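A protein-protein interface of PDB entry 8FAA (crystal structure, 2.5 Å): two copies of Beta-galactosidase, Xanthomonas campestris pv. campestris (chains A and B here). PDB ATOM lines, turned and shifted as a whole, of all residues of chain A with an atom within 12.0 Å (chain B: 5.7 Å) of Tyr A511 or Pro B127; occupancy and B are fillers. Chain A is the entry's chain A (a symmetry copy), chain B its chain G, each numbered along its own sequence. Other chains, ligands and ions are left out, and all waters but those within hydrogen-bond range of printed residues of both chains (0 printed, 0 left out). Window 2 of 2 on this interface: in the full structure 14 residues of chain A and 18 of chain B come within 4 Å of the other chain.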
ATOM      1  N   ASP A 399      -7.761 -27.225  12.315  1.00  0.00           N
ATOM      2  CA  ASP A 399      -8.077 -26.708  10.991  1.00  0.00           C
ATOM      3  C   ASP A 399      -7.079 -25.654  10.515  1.00  0.00           C
ATOM      4  O   ASP A 399      -6.939 -25.450   9.302  1.00  0.00           O
ATOM      5  CB  ASP A 399      -9.487 -26.132  11.008  1.00  0.00           C
ATOM      6  CG  ASP A 399     -10.541 -27.206  11.014  1.00  0.00           C
ATOM      7  OD1 ASP A 399     -11.725 -26.880  11.234  1.00  0.00           O
ATOM      8  OD2 ASP A 399     -10.175 -28.385  10.810  1.00  0.00           O
ATOM      9  N   TRP A 400      -6.386 -24.983  11.433  1.00  0.00           N
ATOM     10  CA  TRP A 400      -5.452 -23.928  11.079  1.00  0.00           C
ATOM     11  C   TRP A 400      -4.021 -24.368  11.354  1.00  0.00           C
ATOM     12  O   TRP A 400      -3.755 -25.142  12.277  1.00  0.00           O
ATOM     13  CB  TRP A 400      -5.760 -22.634  11.842  1.00  0.00           C
ATOM     14  CG  TRP A 400      -6.958 -21.933  11.290  1.00  0.00           C
ATOM     15  CD1 TRP A 400      -8.258 -22.116  11.661  1.00  0.00           C
ATOM     16  CD2 TRP A 400      -6.970 -20.958  10.244  1.00  0.00           C
ATOM     17  NE1 TRP A 400      -9.082 -21.311  10.911  1.00  0.00           N
ATOM     18  CE2 TRP A 400      -8.317 -20.589  10.034  1.00  0.00           C
ATOM     19  CE3 TRP A 400      -5.980 -20.359   9.470  1.00  0.00           C
ATOM     20  CZ2 TRP A 400      -8.692 -19.640   9.085  1.00  0.00           C
ATOM     21  CZ3 TRP A 400      -6.351 -19.421   8.529  1.00  0.00           C
ATOM     22  CH2 TRP A 400      -7.696 -19.067   8.344  1.00  0.00           C
ATOM     23  N   GLU A 436     -10.993 -19.857  16.685  1.00  0.00           N
ATOM     24  CA  GLU A 436     -10.461 -19.076  15.573  1.00  0.00           C
ATOM     25  C   GLU A 436      -9.776 -17.801  16.041  1.00  0.00           C
ATOM     26  O   GLU A 436      -9.794 -16.790  15.330  1.00  0.00           O
ATOM     27  CB  GLU A 436     -11.563 -18.714  14.577  1.00  0.00           C
ATOM     28  CG  GLU A 436     -12.178 -19.902  13.869  1.00  0.00           C
ATOM     29  CD  GLU A 436     -13.294 -19.504  12.937  1.00  0.00           C
ATOM     30  OE1 GLU A 436     -14.192 -18.747  13.368  1.00  0.00           O
ATOM     31  OE2 GLU A 436     -13.266 -19.946  11.768  1.00  0.00           O
ATOM     32  N   PHE A 449      -0.672 -17.807   8.725  1.00  0.00           N
ATOM     33  CA  PHE A 449      -1.731 -18.750   9.052  1.00  0.00           C
ATOM     34  C   PHE A 449      -2.377 -19.294   7.781  1.00  0.00           C
ATOM     35  O   PHE A 449      -2.633 -18.548   6.828  1.00  0.00           O
ATOM     36  CB  PHE A 449      -2.782 -18.092   9.948  1.00  0.00           C
ATOM     37  CG  PHE A 449      -2.316 -17.863  11.368  1.00  0.00           C
ATOM     38  CD1 PHE A 449      -2.470 -18.856  12.330  1.00  0.00           C
ATOM     39  CD2 PHE A 449      -1.737 -16.661  11.742  1.00  0.00           C
ATOM     40  CE1 PHE A 449      -2.047 -18.655  13.643  1.00  0.00           C
ATOM     41  CE2 PHE A 449      -1.316 -16.451  13.048  1.00  0.00           C
ATOM     42  CZ  PHE A 449      -1.473 -17.453  13.998  1.00  0.00           C
ATOM     43  N   PHE A 450      -2.637 -20.604   7.782  1.00  0.00           N
ATOM     44  CA  PHE A 450      -3.222 -21.317   6.652  1.00  0.00           C
ATOM     45  C   PHE A 450      -4.340 -22.219   7.153  1.00  0.00           C
ATOM     46  O   PHE A 450      -4.213 -22.852   8.205  1.00  0.00           O
ATOM     47  CB  PHE A 450      -2.169 -22.159   5.917  1.00  0.00           C
ATOM     48  CG  PHE A 450      -1.105 -21.343   5.232  1.00  0.00           C
ATOM     49  CD1 PHE A 450      -1.370 -20.691   4.037  1.00  0.00           C
ATOM     50  CD2 PHE A 450       0.163 -21.218   5.793  1.00  0.00           C
ATOM     51  CE1 PHE A 450      -0.382 -19.927   3.403  1.00  0.00           C
ATOM     52  CE2 PHE A 450       1.151 -20.464   5.165  1.00  0.00           C
ATOM     53  CZ  PHE A 450       0.876 -19.810   3.968  1.00  0.00           C
ATOM     54  N   ARG A 451      -5.434 -22.277   6.399  1.00  0.00           N
ATOM     55  CA  ARG A 451      -6.573 -23.122   6.722  1.00  0.00           C
ATOM     56  C   ARG A 451      -6.615 -24.308   5.768  1.00  0.00           C
ATOM     57  O   ARG A 451      -6.425 -24.145   4.557  1.00  0.00           O
ATOM     58  CB  ARG A 451      -7.874 -22.326   6.629  1.00  0.00           C
ATOM     59  CG  ARG A 451      -9.062 -22.936   7.339  1.00  0.00           C
ATOM     60  CD  ARG A 451     -10.293 -22.095   7.059  1.00  0.00           C
ATOM     61  NE  ARG A 451     -11.503 -22.581   7.711  1.00  0.00           N
ATOM     62  CZ  ARG A 451     -12.283 -23.544   7.235  1.00  0.00           C
ATOM     63  NH1 ARG A 451     -11.971 -24.205   6.128  1.00  0.00           N
ATOM     64  NH2 ARG A 451     -13.403 -23.851   7.884  1.00  0.00           N
ATOM     65  N   SER A 452      -6.847 -25.505   6.312  1.00  0.00           N
ATOM     66  CA  SER A 452      -7.028 -26.688   5.471  1.00  0.00           C
ATOM     67  C   SER A 452      -8.440 -27.238   5.633  1.00  0.00           C
ATOM     68  O   SER A 452      -9.323 -26.959   4.812  1.00  0.00           O
ATOM     69  CB  SER A 452      -6.002 -27.763   5.818  1.00  0.00           C
ATOM     70  OG  SER A 452      -6.181 -28.201   7.154  1.00  0.00           O
ATOM     71  N   ALA A 453      -8.641 -28.056   6.667  1.00  0.00           N
ATOM     72  CA  ALA A 453      -9.929 -28.350   7.317  1.00  0.00           C
ATOM     73  C   ALA A 453     -10.906 -29.261   6.579  1.00  0.00           C
ATOM     74  O   ALA A 453     -12.033 -29.432   7.088  1.00  0.00           O
ATOM     75  CB  ALA A 453     -10.695 -27.064   7.651  1.00  0.00           C
ATOM     76  N   ALA A 454     -10.550 -29.845   5.428  1.00  0.00           N
ATOM     77  CA  ALA A 454     -11.451 -30.754   4.700  1.00  0.00           C
ATOM     78  C   ALA A 454     -12.801 -30.096   4.408  1.00  0.00           C
ATOM     79  O   ALA A 454     -13.849 -30.750   4.376  1.00  0.00           O
ATOM     80  CB  ALA A 454     -11.638 -32.073   5.455  1.00  0.00           C
ATOM     81  N   ASP A 455     -12.780 -28.783   4.231  1.00  0.00           N
ATOM     82  CA  ASP A 455     -13.905 -28.012   3.746  1.00  0.00           C
ATOM     83  C   ASP A 455     -13.760 -27.808   2.248  1.00  0.00           C
ATOM     84  O   ASP A 455     -12.768 -28.196   1.626  1.00  0.00           O
ATOM     85  CB  ASP A 455     -13.971 -26.651   4.444  1.00  0.00           C
ATOM     86  CG  ASP A 455     -14.579 -26.726   5.812  1.00  0.00           C
ATOM     87  OD1 ASP A 455     -14.848 -25.658   6.397  1.00  0.00           O
ATOM     88  OD2 ASP A 455     -14.794 -27.856   6.295  1.00  0.00           O
ATOM     89  N   THR A 456     -14.762 -27.172   1.662  1.00  0.00           N
ATOM     90  CA  THR A 456     -14.568 -26.439   0.425  1.00  0.00           C
ATOM     91  C   THR A 456     -14.420 -24.947   0.695  1.00  0.00           C
ATOM     92  O   THR A 456     -14.441 -24.147  -0.245  1.00  0.00           O
ATOM     93  CB  THR A 456     -15.725 -26.704  -0.540  1.00  0.00           C
ATOM     94  OG1 THR A 456     -16.967 -26.330   0.071  1.00  0.00           O
ATOM     95  CG2 THR A 456     -15.770 -28.180  -0.891  1.00  0.00           C
ATOM     96  N   ARG A 457     -14.262 -24.570   1.963  1.00  0.00           N
ATOM     97  CA  ARG A 457     -14.173 -23.191   2.414  1.00  0.00           C
ATOM     98  C   ARG A 457     -12.739 -22.676   2.319  1.00  0.00           C
ATOM     99  O   ARG A 457     -11.779 -23.446   2.262  1.00  0.00           O
ATOM    100  CB  ARG A 457     -14.666 -23.078   3.854  1.00  0.00           C
ATOM    101  CG  ARG A 457     -16.095 -23.523   4.041  1.00  0.00           C
ATOM    102  CD  ARG A 457     -16.698 -22.936   5.306  1.00  0.00           C
ATOM    103  NE  ARG A 457     -17.623 -21.853   4.996  1.00  0.00           N
ATOM    104  CZ  ARG A 457     -17.773 -20.769   5.740  1.00  0.00           C
ATOM    105  NH1 ARG A 457     -17.095 -20.608   6.863  1.00  0.00           N
ATOM    106  NH2 ARG A 457     -18.631 -19.827   5.356  1.00  0.00           N
ATOM    107  N   HIS A 458     -12.601 -21.353   2.312  1.00  0.00           N
ATOM    108  CA  HIS A 458     -11.307 -20.704   2.165  1.00  0.00           C
ATOM    109  C   HIS A 458     -11.021 -19.886   3.412  1.00  0.00           C
ATOM    110  O   HIS A 458     -11.917 -19.202   3.916  1.00  0.00           O
ATOM    111  CB  HIS A 458     -11.278 -19.807   0.925  1.00  0.00           C
ATOM    112  CG  HIS A 458     -11.256 -20.563  -0.366  1.00  0.00           C
ATOM    113  ND1 HIS A 458     -10.087 -20.833  -1.052  1.00  0.00           N
ATOM    114  CD2 HIS A 458     -12.257 -21.115  -1.095  1.00  0.00           C
ATOM    115  CE1 HIS A 458     -10.371 -21.510  -2.151  1.00  0.00           C
ATOM    116  NE2 HIS A 458     -11.680 -21.695  -2.201  1.00  0.00           N
ATOM    117  N   GLY A 459      -9.783 -19.960   3.908  1.00  0.00           N
ATOM    118  CA  GLY A 459      -9.422 -19.204   5.096  1.00  0.00           C
ATOM    119  C   GLY A 459      -9.170 -17.740   4.782  1.00  0.00           C
ATOM    120  O   GLY A 459      -8.870 -17.362   3.650  1.00  0.00           O
ATOM    121  N   GLN A 460      -9.315 -16.893   5.801  1.00  0.00           N
ATOM    122  CA  GLN A 460      -9.028 -15.484   5.599  1.00  0.00           C
ATOM    123  C   GLN A 460      -8.796 -14.803   6.934  1.00  0.00           C
ATOM    124  O   GLN A 460      -9.336 -15.205   7.969  1.00  0.00           O
ATOM    125  CB  GLN A 460     -10.149 -14.765   4.839  1.00  0.00           C
ATOM    126  CG  GLN A 460     -11.472 -14.649   5.585  1.00  0.00           C
ATOM    127  CD  GLN A 460     -12.528 -13.910   4.779  1.00  0.00           C
ATOM    128  OE1 GLN A 460     -12.213 -13.194   3.833  1.00  0.00           O
ATOM    129  NE2 GLN A 460     -13.796 -14.112   5.129  1.00  0.00           N
ATOM    130  N   LEU A 461      -7.999 -13.739   6.876  1.00  0.00           N
ATOM    131  CA  LEU A 461      -7.712 -12.904   8.031  1.00  0.00           C
ATOM    132  C   LEU A 461      -8.862 -11.926   8.253  1.00  0.00           C
ATOM    133  O   LEU A 461      -9.198 -11.150   7.354  1.00  0.00           O
ATOM    134  CB  LEU A 461      -6.401 -12.152   7.806  1.00  0.00           C
ATOM    135  CG  LEU A 461      -5.354 -12.170   8.923  1.00  0.00           C
ATOM    136  CD1 LEU A 461      -4.895 -13.587   9.175  1.00  0.00           C
ATOM    137  CD2 LEU A 461      -4.172 -11.328   8.558  1.00  0.00           C
ATOM    138  N   LEU A 462      -9.462 -11.955   9.442  1.00  0.00           N
ATOM    139  CA  LEU A 462     -10.566 -11.065   9.787  1.00  0.00           C
ATOM    140  C   LEU A 462     -10.129  -9.822  10.559  1.00  0.00           C
ATOM    141  O   LEU A 462     -10.518  -8.711  10.189  1.00  0.00           O
ATOM    142  CB  LEU A 462     -11.633 -11.827  10.587  1.00  0.00           C
ATOM    143  CG  LEU A 462     -12.542 -12.762   9.781  1.00  0.00           C
ATOM    144  CD1 LEU A 462     -13.601 -13.385  10.676  1.00  0.00           C
ATOM    145  CD2 LEU A 462     -13.187 -12.036   8.600  1.00  0.00           C
ATOM    146  N   ARG A 507      -7.620 -12.854  14.744  1.00  0.00           N
ATOM    147  CA  ARG A 507      -8.897 -13.527  14.548  1.00  0.00           C
ATOM    148  C   ARG A 507      -9.042 -13.913  13.083  1.00  0.00           C
ATOM    149  O   ARG A 507      -8.847 -13.074  12.198  1.00  0.00           O
ATOM    150  CB  ARG A 507     -10.061 -12.634  14.986  1.00  0.00           C
ATOM    151  CG  ARG A 507     -11.390 -13.355  15.074  1.00  0.00           C
ATOM    152  CD  ARG A 507     -12.340 -12.596  15.971  1.00  0.00           C
ATOM    153  NE  ARG A 507     -12.513 -11.221  15.521  1.00  0.00           N
ATOM    154  CZ  ARG A 507     -13.344 -10.851  14.556  1.00  0.00           C
ATOM    155  NH1 ARG A 507     -14.116 -11.730  13.934  1.00  0.00           N
ATOM    156  NH2 ARG A 507     -13.395  -9.570  14.202  1.00  0.00           N
ATOM    157  N   VAL A 508      -9.380 -15.176  12.829  1.00  0.00           N
ATOM    158  CA  VAL A 508      -9.485 -15.701  11.476  1.00  0.00           C
ATOM    159  C   VAL A 508     -10.921 -16.140  11.214  1.00  0.00           C
ATOM    160  O   VAL A 508     -11.759 -16.190  12.114  1.00  0.00           O
ATOM    161  CB  VAL A 508      -8.502 -16.862  11.213  1.00  0.00           C
ATOM    162  CG1 VAL A 508      -7.080 -16.350  11.148  1.00  0.00           C
ATOM    163  CG2 VAL A 508      -8.626 -17.928  12.288  1.00  0.00           C
ATOM    164  N   GLY A 509     -11.190 -16.453   9.951  1.00  0.00           N
ATOM    165  CA  GLY A 509     -12.497 -16.905   9.528  1.00  0.00           C
ATOM    166  C   GLY A 509     -12.418 -17.576   8.171  1.00  0.00           C
ATOM    167  O   GLY A 509     -11.335 -17.858   7.653  1.00  0.00           O
ATOM    168  N   SER A 510     -13.586 -17.820   7.586  1.00  0.00           N
ATOM    169  CA  SER A 510     -13.658 -18.504   6.304  1.00  0.00           C
ATOM    170  C   SER A 510     -14.793 -17.928   5.469  1.00  0.00           C
ATOM    171  O   SER A 510     -15.586 -17.108   5.933  1.00  0.00           O
ATOM    172  CB  SER A 510     -13.863 -20.008   6.484  1.00  0.00           C
ATOM    173  OG  SER A 510     -14.974 -20.245   7.326  1.00  0.00           O
ATOM    174  N   TYR A 511     -14.862 -18.381   4.220  1.00  0.00           N
ATOM    175  CA  TYR A 511     -15.911 -17.983   3.287  1.00  0.00           C
ATOM    176  C   TYR A 511     -16.097 -19.052   2.233  1.00  0.00           C
ATOM    177  O   TYR A 511     -15.256 -19.946   2.088  1.00  0.00           O
ATOM    178  CB  TYR A 511     -15.580 -16.648   2.608  1.00  0.00           C
ATOM    179  CG  TYR A 511     -14.445 -16.709   1.602  1.00  0.00           C
ATOM    180  CD1 TYR A 511     -14.665 -17.125   0.292  1.00  0.00           C
ATOM    181  CD2 TYR A 511     -13.156 -16.321   1.952  1.00  0.00           C
ATOM    182  CE1 TYR A 511     -13.637 -17.175  -0.630  1.00  0.00           C
ATOM    183  CE2 TYR A 511     -12.124 -16.362   1.034  1.00  0.00           C
ATOM    184  CZ  TYR A 511     -12.368 -16.791  -0.260  1.00  0.00           C
ATOM    185  OH  TYR A 511     -11.347 -16.837  -1.189  1.00  0.00           O
ATOM    186  OXT TYR A 511     -17.070 -19.001   1.483  1.00  0.00           O
ATOM    187  N   LYS B 111     -16.860  -9.524   3.864  1.00  0.00           N
ATOM    188  CA  LYS B 111     -15.945 -10.667   3.853  1.00  0.00           C
ATOM    189  C   LYS B 111     -16.647 -11.971   4.227  1.00  0.00           C
ATOM    190  O   LYS B 111     -16.256 -13.039   3.747  1.00  0.00           O
ATOM    191  CB  LYS B 111     -14.778 -10.420   4.809  1.00  0.00           C
ATOM    192  CG  LYS B 111     -13.655  -9.575   4.226  1.00  0.00           C
ATOM    193  CD  LYS B 111     -12.329  -9.879   4.907  1.00  0.00           C
ATOM    194  CE  LYS B 111     -11.317  -8.759   4.703  1.00  0.00           C
ATOM    195  NZ  LYS B 111     -11.327  -7.793   5.830  1.00  0.00           N
ATOM    196  N   ARG B 112     -17.672 -11.912   5.079  1.00  0.00           N
ATOM    197  CA  ARG B 112     -18.423 -13.107   5.453  1.00  0.00           C
ATOM    198  C   ARG B 112     -19.374 -13.589   4.361  1.00  0.00           C
ATOM    199  O   ARG B 112     -19.797 -14.748   4.399  1.00  0.00           O
ATOM    200  CB  ARG B 112     -19.242 -12.848   6.722  1.00  0.00           C
ATOM    201  CG  ARG B 112     -18.475 -12.200   7.858  1.00  0.00           C
ATOM    202  CD  ARG B 112     -17.368 -13.101   8.397  1.00  0.00           C
ATOM    203  NE  ARG B 112     -17.091 -12.832   9.803  1.00  0.00           N
ATOM    204  CZ  ARG B 112     -17.727 -13.411  10.812  1.00  0.00           C
ATOM    205  NH1 ARG B 112     -18.693 -14.292  10.607  1.00  0.00           N
ATOM    206  NH2 ARG B 112     -17.389 -13.096  12.059  1.00  0.00           N
ATOM    207  N   GLU B 114     -19.655 -14.028   0.616  1.00  0.00           N
ATOM    208  CA  GLU B 114     -19.226 -14.117  -0.774  1.00  0.00           C
ATOM    209  C   GLU B 114     -20.398 -14.320  -1.725  1.00  0.00           C
ATOM    210  O   GLU B 114     -20.269 -14.023  -2.918  1.00  0.00           O
ATOM    211  CB  GLU B 114     -18.214 -15.243  -0.953  1.00  0.00           C
ATOM    212  CG  GLU B 114     -17.181 -14.985  -2.046  1.00  0.00           C
ATOM    213  CD  GLU B 114     -17.529 -15.643  -3.375  1.00  0.00           C
ATOM    214  OE1 GLU B 114     -18.202 -16.698  -3.358  1.00  0.00           O
ATOM    215  OE2 GLU B 114     -17.121 -15.113  -4.436  1.00  0.00           O
ATOM    216  N   ARG B 119     -16.358 -12.622  -5.246  1.00  0.00           N
ATOM    217  CA  ARG B 119     -14.954 -12.435  -5.577  1.00  0.00           C
ATOM    218  C   ARG B 119     -14.691 -12.778  -7.037  1.00  0.00           C
ATOM    219  O   ARG B 119     -15.388 -13.610  -7.629  1.00  0.00           O
ATOM    220  CB  ARG B 119     -14.081 -13.321  -4.683  1.00  0.00           C
ATOM    221  CG  ARG B 119     -14.305 -13.078  -3.209  1.00  0.00           C
ATOM    222  CD  ARG B 119     -13.340 -13.848  -2.333  1.00  0.00           C
ATOM    223  NE  ARG B 119     -13.540 -13.492  -0.935  1.00  0.00           N
ATOM    224  CZ  ARG B 119     -12.558 -13.296  -0.065  1.00  0.00           C
ATOM    225  NH1 ARG B 119     -11.287 -13.437  -0.412  1.00  0.00           N
ATOM    226  NH2 ARG B 119     -12.859 -12.957   1.188  1.00  0.00           N
ATOM    227  N   MET B 120     -13.669 -12.145  -7.618  1.00  0.00           N
ATOM    228  CA  MET B 120     -13.227 -12.580  -8.935  1.00  0.00           C
ATOM    229  C   MET B 120     -12.784 -14.037  -8.881  1.00  0.00           C
ATOM    230  O   MET B 120     -12.320 -14.533  -7.849  1.00  0.00           O
ATOM    231  CB  MET B 120     -12.079 -11.717  -9.474  1.00  0.00           C
ATOM    232  CG  MET B 120     -12.407 -10.245  -9.679  1.00  0.00           C
ATOM    233  SD  MET B 120     -10.954  -9.226 -10.056  1.00  0.00           S
ATOM    234  CE  MET B 120     -10.693  -9.674 -11.764  1.00  0.00           C
ATOM    235  N   ARG B 121     -12.945 -14.729 -10.003  1.00  0.00           N
ATOM    236  CA  ARG B 121     -12.434 -16.079 -10.156  1.00  0.00           C
ATOM    237  C   ARG B 121     -11.237 -16.036 -11.090  1.00  0.00           C
ATOM    238  O   ARG B 121     -11.221 -15.268 -12.058  1.00  0.00           O
ATOM    239  CB  ARG B 121     -13.504 -17.035 -10.704  1.00  0.00           C
ATOM    240  CG  ARG B 121     -14.692 -17.300  -9.774  1.00  0.00           C
ATOM    241  CD  ARG B 121     -14.261 -17.953  -8.464  1.00  0.00           C
ATOM    242  NE  ARG B 121     -15.393 -18.494  -7.717  1.00  0.00           N
ATOM    243  CZ  ARG B 121     -16.199 -17.780  -6.940  1.00  0.00           C
ATOM    244  NH1 ARG B 121     -16.032 -16.473  -6.779  1.00  0.00           N
ATOM    245  NH2 ARG B 121     -17.197 -18.389  -6.306  1.00  0.00           N
ATOM    246  N   ASP B 122     -10.229 -16.847 -10.794  1.00  0.00           N
ATOM    247  CA  ASP B 122      -9.040 -16.866 -11.628  1.00  0.00           C
ATOM    248  C   ASP B 122      -9.225 -17.860 -12.769  1.00  0.00           C
ATOM    249  O   ASP B 122     -10.280 -18.483 -12.925  1.00  0.00           O
ATOM    250  CB  ASP B 122      -7.792 -17.132 -10.773  1.00  0.00           C
ATOM    251  CG  ASP B 122      -7.780 -18.506 -10.093  1.00  0.00           C
ATOM    252  OD1 ASP B 122      -8.647 -19.362 -10.369  1.00  0.00           O
ATOM    253  OD2 ASP B 122      -6.908 -18.713  -9.221  1.00  0.00           O
ATOM    254  N   GLY B 125     -10.708 -21.185 -11.987  1.00  0.00           N
ATOM    255  CA  GLY B 125     -12.008 -21.201 -11.339  1.00  0.00           C
ATOM    256  C   GLY B 125     -11.999 -20.968  -9.846  1.00  0.00           C
ATOM    257  O   GLY B 125     -13.052 -21.092  -9.208  1.00  0.00           O
ATOM    258  N   GLU B 126     -10.856 -20.626  -9.271  1.00  0.00           N
ATOM    259  CA  GLU B 126     -10.605 -20.405  -7.854  1.00  0.00           C
ATOM    260  C   GLU B 126     -10.832 -18.938  -7.498  1.00  0.00           C
ATOM    261  O   GLU B 126     -10.524 -18.053  -8.301  1.00  0.00           O
ATOM    262  CB  GLU B 126      -9.176 -20.805  -7.503  1.00  0.00           C
ATOM    263  CG  GLU B 126      -8.946 -22.304  -7.441  1.00  0.00           C
ATOM    264  CD  GLU B 126      -9.914 -23.003  -6.513  1.00  0.00           C
ATOM    265  OE1 GLU B 126     -10.675 -23.874  -6.990  1.00  0.00           O
ATOM    266  OE2 GLU B 126      -9.913 -22.670  -5.305  1.00  0.00           O
ATOM    267  N   PRO B 127     -11.376 -18.657  -6.316  1.00  0.00           N
ATOM    268  CA  PRO B 127     -11.495 -17.265  -5.877  1.00  0.00           C
ATOM    269  C   PRO B 127     -10.127 -16.663  -5.609  1.00  0.00           C
ATOM    270  O   PRO B 127      -9.138 -17.362  -5.390  1.00  0.00           O
ATOM    271  CB  PRO B 127     -12.321 -17.354  -4.589  1.00  0.00           C
ATOM    272  CG  PRO B 127     -12.780 -18.779  -4.498  1.00  0.00           C
ATOM    273  CD  PRO B 127     -11.810 -19.597  -5.274  1.00  0.00           C
ATOM    274  N   VAL B 128     -10.080 -15.337  -5.678  1.00  0.00           N
ATOM    275  CA  VAL B 128      -8.938 -14.536  -5.275  1.00  0.00           C
ATOM    276  C   VAL B 128      -9.441 -13.439  -4.343  1.00  0.00           C
ATOM    277  O   VAL B 128     -10.639 -13.318  -4.090  1.00  0.00           O
ATOM    278  CB  VAL B 128      -8.173 -13.939  -6.478  1.00  0.00           C
ATOM    279  CG1 VAL B 128      -7.431 -15.031  -7.239  1.00  0.00           C
ATOM    280  CG2 VAL B 128      -9.123 -13.198  -7.400  1.00  0.00           C
ATOM    281  N   ASP B 129      -8.512 -12.646  -3.826  1.00  0.00           N
ATOM    282  CA  ASP B 129      -8.849 -11.631  -2.831  1.00  0.00           C
ATOM    283  C   ASP B 129      -9.204 -10.299  -3.486  1.00  0.00           C
ATOM    284  O   ASP B 129      -8.701  -9.239  -3.114  1.00  0.00           O
ATOM    285  CB  ASP B 129      -7.702 -11.470  -1.836  1.00  0.00           C
ATOM    286  CG  ASP B 129      -7.512 -12.693  -0.962  1.00  0.00           C
ATOM    287  OD1 ASP B 129      -8.359 -13.609  -1.015  1.00  0.00           O
ATOM    288  OD2 ASP B 129      -6.532 -12.725  -0.193  1.00  0.00           O
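Of the 22 printed residues of chain A, 4 touch a printed residue of chain B. Hydrophobic or aromatic side chains of chain A within 4 Å of the printed part of chain B: His A458, Leu A462 and Tyr A511. Hydrophobic or aromatic side chains of chain B within 4 Å of the printed part of chain A: Pro B127.
Phe A449 touches none of the printed residues of chain B. Of the printed residues of chain B, Leu A462 touches Arg B112 (3.6 Å). Tyr A511 touches just these residues of chain B: Lys B111 (3.8 Å), Arg B119 (3.3 Å) and Pro B127 (3.6 Å). Printed residues of chain A within 4 Å of Lys B111: Gln A460 (3.0 Å) and Tyr A511 (3.8 Å). Of the printed residues of chain A, Arg B112 touches Leu A462. Glu B114 touches none of the printed residues of chain A. No residue of chain A comes within 4 Å of Arg B121. No residue of chain A comes within 4 Å of Gly B125. Pro B127 touches just these residues of chain A: His A458 (3.7 Å) and Tyr A511 (3.6 Å). No residue of chain A comes within 4 Å of Val B128. The nearest residue of chain A that does not touch Pro B127 is Thr A456 (7.0 Å).
OD1 of Asp B122 sits at hydrogen-bond distance from N of Glu B126, 2.8 Å away. The backbone NH (N) of Gln A460 sits at hydrogen-bond distance from the backbone carbonyl oxygen (O) of Gly A509. The backbone NH (N) of His A458 lies within hydrogen-bond range of the chain-end carboxylate (O) of Tyr A511 (3.0 Å). The guanidinium group of Arg B119 lies within salt-bridge range of the side-chain carboxylate of Asp B129 (3.0 Å). The backbone carbonyl oxygen (O) of Arg A507 sits at hydrogen-bond distance from the backbone NH (N) of Leu A462 (3.0 Å). The backbone NH of Arg B119 is in hydrogen-bond range of the side-chain carboxylate of Glu B114, 2.7 Å away.
Glu B126 touches His A458. His A458 touches Pro B127 (NE2 to CD, 3.7 Å). Leu A462 touches Arg B112 (CD1 to NE, 3.6 Å). Tyr A511 touches Lys B111. Pro B127 touches Tyr A511 (CB to OH, 3.6 Å).
No position is printed for both chains.
The guanidinium group (NH1) of Arg B119 lies close to the side-chain hydroxyl (OH) of Tyr A511 (3.5 Å). NE2 of Gln A460 sits at hydrogen-bond distance from O of Lys B111, 3.0 Å away. The guanidinium group of Arg B119 is in hydrogen-bond range of the side-chain amide oxygen of Gln A460, 2.7 Å away.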
